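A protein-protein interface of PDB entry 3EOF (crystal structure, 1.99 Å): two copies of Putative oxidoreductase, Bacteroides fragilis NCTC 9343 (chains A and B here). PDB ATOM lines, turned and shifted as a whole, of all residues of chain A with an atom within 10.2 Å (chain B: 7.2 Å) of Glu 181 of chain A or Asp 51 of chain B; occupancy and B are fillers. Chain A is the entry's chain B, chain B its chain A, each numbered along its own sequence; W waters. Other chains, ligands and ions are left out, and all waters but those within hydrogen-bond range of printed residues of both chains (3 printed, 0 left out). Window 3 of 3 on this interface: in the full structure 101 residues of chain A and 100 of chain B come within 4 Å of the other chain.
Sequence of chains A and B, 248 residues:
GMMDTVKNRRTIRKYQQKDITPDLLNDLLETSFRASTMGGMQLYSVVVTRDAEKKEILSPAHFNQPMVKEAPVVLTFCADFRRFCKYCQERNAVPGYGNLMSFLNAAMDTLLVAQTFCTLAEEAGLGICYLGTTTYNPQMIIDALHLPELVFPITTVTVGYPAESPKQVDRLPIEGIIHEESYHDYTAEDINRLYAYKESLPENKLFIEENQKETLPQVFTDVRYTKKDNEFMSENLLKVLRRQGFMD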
ATOM      1  N   ILE A 177       0.755  14.399   6.556  1.00  0.00           N
ATOM      2  CA  ILE A 177       1.669  14.013   5.467  1.00  0.00           C
ATOM      3  C   ILE A 177       1.591  12.543   5.128  1.00  0.00           C
ATOM      4  O   ILE A 177       1.710  12.167   3.985  1.00  0.00           O
ATOM      5  CB  ILE A 177       3.144  14.303   5.877  1.00  0.00           C
ATOM      6  CG1 ILE A 177       3.348  15.758   6.350  1.00  0.00           C
ATOM      7  CG2 ILE A 177       4.080  13.954   4.750  1.00  0.00           C
ATOM      8  CD1 ILE A 177       3.074  16.811   5.271  1.00  0.00           C
ATOM      9  N   ILE A 178       1.408  11.702   6.143  1.00  0.00           N
ATOM     10  CA  ILE A 178       1.341  10.255   5.979  1.00  0.00           C
ATOM     11  C   ILE A 178      -0.103   9.829   5.763  1.00  0.00           C
ATOM     12  O   ILE A 178      -0.999  10.267   6.499  1.00  0.00           O
ATOM     13  CB  ILE A 178       1.917   9.526   7.231  1.00  0.00           C
ATOM     14  CG1 ILE A 178       3.369   9.961   7.454  1.00  0.00           C
ATOM     15  CG2 ILE A 178       1.764   7.998   7.098  1.00  0.00           C
ATOM     16  CD1 ILE A 178       3.983   9.567   8.811  1.00  0.00           C
ATOM     17  N   HIS A 179      -0.277   8.960   4.763  1.00  0.00           N
ATOM     18  CA  HIS A 179      -1.546   8.358   4.348  1.00  0.00           C
ATOM     19  C   HIS A 179      -1.411   6.838   4.415  1.00  0.00           C
ATOM     20  O   HIS A 179      -0.483   6.265   3.838  1.00  0.00           O
ATOM     21  CB  HIS A 179      -1.889   8.749   2.906  1.00  0.00           C
ATOM     22  CG  HIS A 179      -1.961  10.236   2.691  1.00  0.00           C
ATOM     23  ND1 HIS A 179      -3.152  10.915   2.594  1.00  0.00           N
ATOM     24  CD2 HIS A 179      -0.989  11.169   2.582  1.00  0.00           C
ATOM     25  CE1 HIS A 179      -2.912  12.207   2.446  1.00  0.00           C
ATOM     26  NE2 HIS A 179      -1.608  12.388   2.417  1.00  0.00           N
ATOM     27  N   GLU A 180      -2.339   6.183   5.108  1.00  0.00           N
ATOM     28  CA  GLU A 180      -2.290   4.732   5.248  1.00  0.00           C
ATOM     29  C   GLU A 180      -3.025   4.076   4.083  1.00  0.00           C
ATOM     30  O   GLU A 180      -4.236   4.287   3.905  1.00  0.00           O
ATOM     31  CB  GLU A 180      -2.884   4.306   6.592  1.00  0.00           C
ATOM     32  CG  GLU A 180      -2.108   4.897   7.825  1.00  0.00           C
ATOM     33  CD  GLU A 180      -2.739   4.537   9.204  1.00  0.00           C
ATOM     34  OE1 GLU A 180      -3.618   3.627   9.273  1.00  0.00           O
ATOM     35  OE2 GLU A 180      -2.345   5.172  10.211  1.00  0.00           O
ATOM     36  N   GLU A 181      -2.262   3.331   3.279  1.00  0.00           N
ATOM     37  CA  GLU A 181      -2.747   2.539   2.134  1.00  0.00           C
ATOM     38  C   GLU A 181      -3.282   3.294   0.933  1.00  0.00           C
ATOM     39  O   GLU A 181      -3.154   2.817  -0.187  1.00  0.00           O
ATOM     40  CB  GLU A 181      -3.794   1.501   2.551  1.00  0.00           C
ATOM     41  CG  GLU A 181      -3.362   0.544   3.627  1.00  0.00           C
ATOM     42  CD  GLU A 181      -2.155  -0.285   3.282  1.00  0.00           C
ATOM     43  OE1 GLU A 181      -1.914  -0.574   2.084  1.00  0.00           O
ATOM     44  OE2 GLU A 181      -1.432  -0.638   4.238  1.00  0.00           O
ATOM     45  N   SER A 182      -3.952   4.413   1.176  1.00  0.00           N
ATOM     46  CA  SER A 182      -4.469   5.253   0.115  1.00  0.00           C
ATOM     47  C   SER A 182      -4.487   6.708   0.581  1.00  0.00           C
ATOM     48  O   SER A 182      -4.428   7.016   1.756  1.00  0.00           O
ATOM     49  CB  SER A 182      -5.873   4.816  -0.299  1.00  0.00           C
ATOM     50  OG  SER A 182      -6.788   5.141   0.722  1.00  0.00           O
ATOM     51  N   TYR A 183      -4.565   7.598  -0.385  1.00  0.00           N
ATOM     52  CA  TYR A 183      -4.582   9.030  -0.140  1.00  0.00           C
ATOM     53  C   TYR A 183      -5.904   9.399   0.504  1.00  0.00           C
ATOM     54  O   TYR A 183      -6.949   9.084  -0.011  1.00  0.00           O
ATOM     55  CB  TYR A 183      -4.356   9.777  -1.466  1.00  0.00           C
ATOM     56  CG  TYR A 183      -4.010  11.224  -1.319  1.00  0.00           C
ATOM     57  CD1 TYR A 183      -5.001  12.185  -1.200  1.00  0.00           C
ATOM     58  CD2 TYR A 183      -2.710  11.635  -1.331  1.00  0.00           C
ATOM     59  CE1 TYR A 183      -4.691  13.490  -1.073  1.00  0.00           C
ATOM     60  CE2 TYR A 183      -2.385  12.936  -1.196  1.00  0.00           C
ATOM     61  CZ  TYR A 183      -3.383  13.861  -1.070  1.00  0.00           C
ATOM     62  OH  TYR A 183      -3.074  15.163  -0.939  1.00  0.00           O
ATOM     63  N   HIS A 184      -5.839   9.994   1.687  1.00  0.00           N
ATOM     64  CA  HIS A 184      -7.009  10.487   2.363  1.00  0.00           C
ATOM     65  C   HIS A 184      -7.020  12.006   2.196  1.00  0.00           C
ATOM     66  O   HIS A 184      -6.252  12.768   2.828  1.00  0.00           O
ATOM     67  CB  HIS A 184      -7.033  10.020   3.810  1.00  0.00           C
ATOM     68  CG  HIS A 184      -7.160   8.533   3.928  1.00  0.00           C
ATOM     69  ND1 HIS A 184      -6.093   7.711   4.213  1.00  0.00           N
ATOM     70  CD2 HIS A 184      -8.219   7.713   3.717  1.00  0.00           C
ATOM     71  CE1 HIS A 184      -6.492   6.452   4.204  1.00  0.00           C
ATOM     72  NE2 HIS A 184      -7.777   6.424   3.905  1.00  0.00           N
ATOM     73  N   VAL B  46       3.215  10.892   1.736  1.00  0.00           N
ATOM     74  CA  VAL B  46       3.774   9.559   1.738  1.00  0.00           C
ATOM     75  C   VAL B  46       2.632   8.583   1.966  1.00  0.00           C
ATOM     76  O   VAL B  46       1.963   8.596   3.038  1.00  0.00           O
ATOM     77  CB  VAL B  46       4.822   9.376   2.883  1.00  0.00           C
ATOM     78  CG1 VAL B  46       5.495   7.953   2.776  1.00  0.00           C
ATOM     79  CG2 VAL B  46       5.874  10.519   2.884  1.00  0.00           C
ATOM     80  N   VAL B  47       2.378   7.730   0.975  1.00  0.00           N
ATOM     81  CA  VAL B  47       1.437   6.667   1.155  1.00  0.00           C
ATOM     82  C   VAL B  47       2.213   5.460   1.689  1.00  0.00           C
ATOM     83  O   VAL B  47       3.190   4.995   1.075  1.00  0.00           O
ATOM     84  CB  VAL B  47       0.679   6.297  -0.129  1.00  0.00           C
ATOM     85  CG1 VAL B  47      -0.298   5.229   0.187  1.00  0.00           C
ATOM     86  CG2 VAL B  47      -0.028   7.513  -0.681  1.00  0.00           C
ATOM     87  N   VAL B  48       1.774   4.976   2.848  1.00  0.00           N
ATOM     88  CA  VAL B  48       2.340   3.808   3.538  1.00  0.00           C
ATOM     89  C   VAL B  48       1.447   2.599   3.230  1.00  0.00           C
ATOM     90  O   VAL B  48       0.278   2.594   3.575  1.00  0.00           O
ATOM     91  CB  VAL B  48       2.413   4.022   5.066  1.00  0.00           C
ATOM     92  CG1 VAL B  48       2.939   2.749   5.785  1.00  0.00           C
ATOM     93  CG2 VAL B  48       3.284   5.287   5.397  1.00  0.00           C
ATOM     94  N   THR B  49       2.030   1.625   2.516  1.00  0.00           N
ATOM     95  CA  THR B  49       1.437   0.356   2.148  1.00  0.00           C
ATOM     96  C   THR B  49       2.020  -0.828   2.938  1.00  0.00           C
ATOM     97  O   THR B  49       3.165  -1.186   2.794  1.00  0.00           O
ATOM     98  CB  THR B  49       1.649   0.138   0.676  1.00  0.00           C
ATOM     99  OG1 THR B  49       1.020   1.231  -0.012  1.00  0.00           O
ATOM    100  CG2 THR B  49       1.131  -1.224   0.207  1.00  0.00           C
ATOM    101  N   ARG B  50       1.194  -1.421   3.781  1.00  0.00           N
ATOM    102  CA  ARG B  50       1.577  -2.556   4.613  1.00  0.00           C
ATOM    103  C   ARG B  50       0.720  -3.792   4.310  1.00  0.00           C
ATOM    104  O   ARG B  50       1.195  -4.904   4.426  1.00  0.00           O
ATOM    105  CB  ARG B  50       1.406  -2.191   6.087  1.00  0.00           C
ATOM    106  CG  ARG B  50       2.358  -1.158   6.622  1.00  0.00           C
ATOM    107  CD  ARG B  50       1.973  -0.943   8.043  1.00  0.00           C
ATOM    108  NE  ARG B  50       2.874  -0.122   8.832  1.00  0.00           N
ATOM    109  CZ  ARG B  50       3.963  -0.564   9.444  1.00  0.00           C
ATOM    110  NH1 ARG B  50       4.362  -1.821   9.292  1.00  0.00           N
ATOM    111  NH2 ARG B  50       4.689   0.279  10.162  1.00  0.00           N
ATOM    112  N   ASP B  51      -0.523  -3.574   3.892  1.00  0.00           N
ATOM    113  CA  ASP B  51      -1.450  -4.650   3.585  1.00  0.00           C
ATOM    114  C   ASP B  51      -0.986  -5.501   2.408  1.00  0.00           C
ATOM    115  O   ASP B  51      -0.581  -4.963   1.384  1.00  0.00           O
ATOM    116  CB  ASP B  51      -2.833  -4.080   3.262  1.00  0.00           C
ATOM    117  CG  ASP B  51      -3.869  -5.168   3.036  1.00  0.00           C
ATOM    118  OD1 ASP B  51      -4.117  -5.943   3.992  1.00  0.00           O
ATOM    119  OD2 ASP B  51      -4.427  -5.258   1.919  1.00  0.00           O
ATOM    120  N   ALA B  52      -1.122  -6.826   2.544  1.00  0.00           N
ATOM    121  CA  ALA B  52      -0.682  -7.780   1.523  1.00  0.00           C
ATOM    122  C   ALA B  52      -1.394  -7.629   0.213  1.00  0.00           C
ATOM    123  O   ALA B  52      -0.756  -7.717  -0.844  1.00  0.00           O
ATOM    124  CB  ALA B  52      -0.816  -9.250   2.013  1.00  0.00           C
ATOM    125  N   GLU B  53      -2.714  -7.446   0.242  1.00  0.00           N
ATOM    126  CA  GLU B  53      -3.453  -7.282  -1.034  1.00  0.00           C
ATOM    127  C   GLU B  53      -3.140  -5.926  -1.649  1.00  0.00           C
ATOM    128  O   GLU B  53      -3.239  -5.771  -2.848  1.00  0.00           O
ATOM    129  CB  GLU B  53      -4.974  -7.445  -0.887  1.00  0.00           C
ATOM    130  CG  GLU B  53      -5.768  -7.225  -2.233  1.00  0.00           C
ATOM    131  N   LYS B  54      -2.769  -4.942  -0.830  1.00  0.00           N
ATOM    132  CA  LYS B  54      -2.437  -3.618  -1.356  1.00  0.00           C
ATOM    133  C   LYS B  54      -1.111  -3.724  -2.098  1.00  0.00           C
ATOM    134  O   LYS B  54      -0.923  -3.103  -3.149  1.00  0.00           O
ATOM    135  CB  LYS B  54      -2.387  -2.553  -0.232  1.00  0.00           C
ATOM    136  CG  LYS B  54      -3.773  -2.157   0.359  1.00  0.00           C
ATOM    137  CD  LYS B  54      -4.701  -1.544  -0.684  1.00  0.00           C
ATOM    138  CE  LYS B  54      -5.904  -0.903  -0.019  1.00  0.00           C
ATOM    139  NZ  LYS B  54      -6.785  -0.192  -1.000  1.00  0.00           N
ATOM    140  N   LYS B  55      -0.192  -4.512  -1.529  1.00  0.00           N
ATOM    141  CA  LYS B  55       1.096  -4.821  -2.166  1.00  0.00           C
ATOM    142  C   LYS B  55       0.910  -5.569  -3.497  1.00  0.00           C
ATOM    143  O   LYS B  55       1.598  -5.307  -4.470  1.00  0.00           O
ATOM    144  CB  LYS B  55       1.962  -5.626  -1.218  1.00  0.00           C
ATOM    145  CG  LYS B  55       2.491  -4.790  -0.078  1.00  0.00           C
ATOM    146  CD  LYS B  55       3.004  -5.625   1.078  1.00  0.00           C
ATOM    147  CE  LYS B  55       3.638  -4.697   2.108  1.00  0.00           C
ATOM    148  NZ  LYS B  55       4.044  -5.447   3.291  1.00  0.00           N
ATOM    149  N   GLU B  56      -0.015  -6.507  -3.530  1.00  0.00           N
ATOM    150  CA  GLU B  56      -0.297  -7.263  -4.750  1.00  0.00           C
ATOM    151  C   GLU B  56      -0.850  -6.366  -5.850  1.00  0.00           C
ATOM    152  O   GLU B  56      -0.577  -6.591  -7.033  1.00  0.00           O
ATOM    153  CB  GLU B  56      -1.256  -8.425  -4.469  1.00  0.00           C
ATOM    154  CG  GLU B  56      -0.564  -9.665  -3.938  1.00  0.00           C
ATOM    155  CD  GLU B  56      -1.528 -10.663  -3.321  1.00  0.00           C
ATOM    156  OE1 GLU B  56      -2.780 -10.504  -3.454  1.00  0.00           O
ATOM    157  OE2 GLU B  56      -1.006 -11.614  -2.684  1.00  0.00           O
ATOM    158  N   ILE B  57      -1.650  -5.377  -5.450  1.00  0.00           N
ATOM    159  CA  ILE B  57      -2.189  -4.373  -6.369  1.00  0.00           C
ATOM    160  C   ILE B  57      -1.091  -3.444  -6.931  1.00  0.00           C
ATOM    161  O   ILE B  57      -1.075  -3.173  -8.122  1.00  0.00           O
ATOM    162  CB  ILE B  57      -3.325  -3.572  -5.702  1.00  0.00           C
ATOM    163  CG1 ILE B  57      -4.547  -4.486  -5.494  1.00  0.00           C
ATOM    164  CG2 ILE B  57      -3.701  -2.408  -6.557  1.00  0.00           C
ATOM    165  CD1 ILE B  57      -5.594  -3.847  -4.621  1.00  0.00           C
ATOM    166  N   LEU B  58      -0.167  -3.002  -6.084  1.00  0.00           N
ATOM    167  CA  LEU B  58       0.974  -2.150  -6.500  1.00  0.00           C
ATOM    168  C   LEU B  58       2.012  -2.863  -7.322  1.00  0.00           C
ATOM    169  O   LEU B  58       2.732  -2.250  -8.088  1.00  0.00           O
ATOM    170  CB  LEU B  58       1.727  -1.579  -5.283  1.00  0.00           C
ATOM    171  CG  LEU B  58       1.147  -0.401  -4.519  1.00  0.00           C
ATOM    172  CD1 LEU B  58       2.155   0.032  -3.430  1.00  0.00           C
ATOM    173  CD2 LEU B  58       0.836   0.738  -5.543  1.00  0.00           C
ATOM    174  N   VAL B  68       8.184  -5.472  -3.709  1.00  0.00           N
ATOM    175  CA  VAL B  68       6.889  -4.888  -3.366  1.00  0.00           C
ATOM    176  C   VAL B  68       6.061  -5.799  -2.439  1.00  0.00           C
ATOM    177  O   VAL B  68       5.383  -5.314  -1.539  1.00  0.00           O
ATOM    178  CB  VAL B  68       6.020  -4.554  -4.608  1.00  0.00           C
ATOM    179  CG1 VAL B  68       4.687  -3.975  -4.144  1.00  0.00           C
ATOM    180  CG2 VAL B  68       6.739  -3.562  -5.541  1.00  0.00           C
ATOM    181  N   PRO B  72       7.967  -5.596   4.316  1.00  0.00           N
ATOM    182  CA  PRO B  72       6.875  -5.339   5.212  1.00  0.00           C
ATOM    183  C   PRO B  72       6.200  -3.987   4.945  1.00  0.00           C
ATOM    184  O   PRO B  72       4.974  -3.844   5.158  1.00  0.00           O
ATOM    185  CB  PRO B  72       7.546  -5.340   6.587  1.00  0.00           C
ATOM    186  CG  PRO B  72       8.913  -4.996   6.349  1.00  0.00           C
ATOM    187  CD  PRO B  72       9.234  -5.699   5.061  1.00  0.00           C
ATOM    188  N   VAL B  74       6.027  -0.656   2.031  1.00  0.00           N
ATOM    189  CA  VAL B  74       6.235  -0.042   0.720  1.00  0.00           C
ATOM    190  C   VAL B  74       5.764   1.390   0.894  1.00  0.00           C
ATOM    191  O   VAL B  74       4.630   1.634   1.320  1.00  0.00           O
ATOM    192  CB  VAL B  74       5.446  -0.757  -0.415  1.00  0.00           C
ATOM    193  CG1 VAL B  74       5.708  -0.098  -1.769  1.00  0.00           C
ATOM    194  CG2 VAL B  74       5.842  -2.216  -0.434  1.00  0.00           C
ATOM    195  N   ALA B 144      -4.169   3.098  -7.969  1.00  0.00           N
ATOM    196  CA  ALA B 144      -4.074   2.181  -6.822  1.00  0.00           C
ATOM    197  C   ALA B 144      -4.198   2.881  -5.486  1.00  0.00           C
ATOM    198  O   ALA B 144      -4.932   2.395  -4.602  1.00  0.00           O
ATOM    199  CB  ALA B 144      -2.783   1.341  -6.889  1.00  0.00           C
ATOM    200  N   LEU B 145      -3.532   4.030  -5.367  1.00  0.00           N
ATOM    201  CA  LEU B 145      -3.464   4.766  -4.105  1.00  0.00           C
ATOM    202  C   LEU B 145      -4.460   5.909  -4.043  1.00  0.00           C
ATOM    203  O   LEU B 145      -4.493   6.656  -3.069  1.00  0.00           O
ATOM    204  CB  LEU B 145      -2.048   5.279  -3.866  1.00  0.00           C
ATOM    205  CG  LEU B 145      -0.945   4.217  -4.001  1.00  0.00           C
ATOM    206  CD1 LEU B 145       0.403   4.804  -3.735  1.00  0.00           C
ATOM    207  CD2 LEU B 145      -1.235   3.007  -3.092  1.00  0.00           C
ATOM    208  N   HIS B 146      -5.275   6.033  -5.084  1.00  0.00           N
ATOM    209  CA  HIS B 146      -6.275   7.081  -5.125  1.00  0.00           C
ATOM    210  C   HIS B 146      -5.699   8.495  -4.969  1.00  0.00           C
ATOM    211  O   HIS B 146      -6.239   9.322  -4.239  1.00  0.00           O
ATOM    212  CB  HIS B 146      -7.350   6.815  -4.051  1.00  0.00           C
ATOM    213  CG  HIS B 146      -7.988   5.472  -4.188  1.00  0.00           C
ATOM    214  ND1 HIS B 146      -7.837   4.474  -3.252  1.00  0.00           N
ATOM    215  CD2 HIS B 146      -8.726   4.940  -5.192  1.00  0.00           C
ATOM    216  CE1 HIS B 146      -8.488   3.395  -3.654  1.00  0.00           C
ATOM    217  NE2 HIS B 146      -9.037   3.653  -4.828  1.00  0.00           N
HETATM  218  O   HOH W   1      -8.016  10.356  -2.506  1.00  0.00           O
HETATM  219  O   HOH W   2      -1.565   0.711  -0.508  1.00  0.00           O
HETATM  220  O   HOH W   3      -5.372   2.103  -1.860  1.00  0.00           O
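N of Thr 49 of chain B is in hydrogen-bond range of O of Val 74 of chain B (2.9 Å).
The backbone carbonyl oxygen (O) of Arg 50 of chain B is in hydrogen-bond range of the side-chain amino group (NZ) of Lys 55 of chain B.
The backbone NH (N) of Glu 53 of chain B sits at hydrogen-bond distance from the side-chain carboxylate (OD2) of Asp 51 of chain B (3.2 Å).
The backbone NH (N) of Lys 54 of chain B sits at hydrogen-bond distance from the side-chain carboxylate (OD2) of Asp 51 of chain B (3.2 Å).
ND1 of His 179 of chain A lies within hydrogen-bond range of N of His 184 of chain A (3.0 Å).
The backbone carbonyl oxygen (O) of Ser 182 of chain A is in hydrogen-bond range of a ring nitrogen (ND1) of His 184 of chain A, at 3.0 Å.
The backbone NH of Val 46 of chain B lies within hydrogen-bond range of the backbone carbonyl oxygen of Ile 177 of chain A, at 3.0 Å.
The backbone NH (N) of His 179 of chain A lies within hydrogen-bond range of the backbone carbonyl oxygen (O) of Val 46 of chain B, 2.9 Å away.
N of Val 48 of chain B lies within hydrogen-bond range of O of His 179 of chain A (2.8 Å).
The backbone NH (N) of Glu 181 of chain A sits at hydrogen-bond distance from the backbone carbonyl oxygen (O) of Val 48 of chain B (2.7 Å).
The side-chain carboxylate (OE2) of Glu 181 of chain A is in hydrogen-bond range of the backbone NH (N) of Arg 50 of chain B.
The backbone NH of Asp 51 of chain B lies within hydrogen-bond range of the side-chain carboxylate of Glu 181 of chain A (3.1 Å).
O of Leu 145 of chain B sits at hydrogen-bond distance from N of Tyr 183 of chain A.
Along chain A the printed residues that touch a printed residue of chain B span positions 177 to 183.
Of the 19 printed residues of chain B, 9 touch a printed residue of chain A.
Hydrophobic or aromatic side chains of chain B that line the printed part of chain A: Val 47, Val 48, Leu 145 and His 146.
Along chain B the printed residues that touch a printed residue of chain A span positions 46 to 146.
Ile 178 of chain A touches Val 48 of chain B (CG2 to CG2, 3.5 Å).
Val 47 of chain B touches His 179 of chain A.
Glu 180 of chain A touches Val 48 of chain B.
CG1 of Val 47 of chain B touches C of Glu 181 of chain A, 3.6 Å away.
Glu 181 of chain A touches Thr 49 of chain B.
CG of Lys 54 of chain B touches OE1 of Glu 181 of chain A (3.0 Å).
Glu 181 of chain A touches Leu 145 of chain B.
Leu 145 of chain B touches Ser 182 of chain A.
Ser 182 of chain A touches His 146 of chain B.
O of His 146 of chain B touches CB of Tyr 183 of chain A, 3.4 Å away.
No position is printed for both chains.
Of the 19 pairs that touch across the chains among the printed residues, none has its exchanged pair printed and touching as well.
Water W2 lies within hydrogen-bond range of the backbone carbonyl oxygen of Glu 181 of chain A (2.7 Å) and the side-chain hydroxyl of Thr 49 of chain B (2.7 Å).
Water W1 bridges O of His 146 of chain B and O of Tyr 183 of chain A.
Water W3 lies within hydrogen-bond range of O of Ala 144 of chain B (2.8 Å), NZ of Lys 54 of chain B (2.8 Å) and O of Glu 181 of chain A (2.9 Å).
Glu 181 of chain A touches just these residues of chain B: Val 47 (3.6 Å), Val 48 (2.7 Å), Thr 49 (3.5 Å), Arg 50 (2.8 Å), Asp 51 (3.1 Å), Lys 54 (3.0 Å) and Leu 145 (3.5 Å).
Printed residues of chain A within 4 Å of Thr 49 of chain B: Glu 181.
No residue of chain A comes within 4 Å of Ala 52 of chain B.
No residue of chain A comes within 4 Å of Glu 53 of chain B.
Lys 54 of chain B touches one residue of chain A.
Of chain A, only Glu 181, Ser 182 and Tyr 183 come within 4 Å of Leu 145 of chain B.
Of the printed residues of chain B, Ile 178 of chain A touches Val 46 and Val 48.
Of the printed residues of chain B, Ile 177 of chain A touches Val 46 (3.0 Å).
Printed residues of chain A within 4 Å of Val 46 of chain B: Ile 177 (3.0 Å), Ile 178 (3.4 Å) and His 179 (2.9 Å).
Of the printed residues of chain A, Arg 50 of chain B touches Glu 181 (2.8 Å).
Of the printed residues of chain A, His 146 of chain B touches Ser 182 and Tyr 183.
Leu 58 of chain B touches none of the printed residues of chain A.
Val 68 of chain B touches none of the printed residues of chain A.
The nearest residue of chain B that does not touch Glu 181 of chain A is Ala 144 of chain B (4.8 Å).
The nearest residue of chain A that does not touch Asp 51 of chain B is Glu 180 of chain A (8.1 Å).
The nearest printed residue of chain B that does not touch His 179 of chain A is Thr 49 of chain B (5.4 Å).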
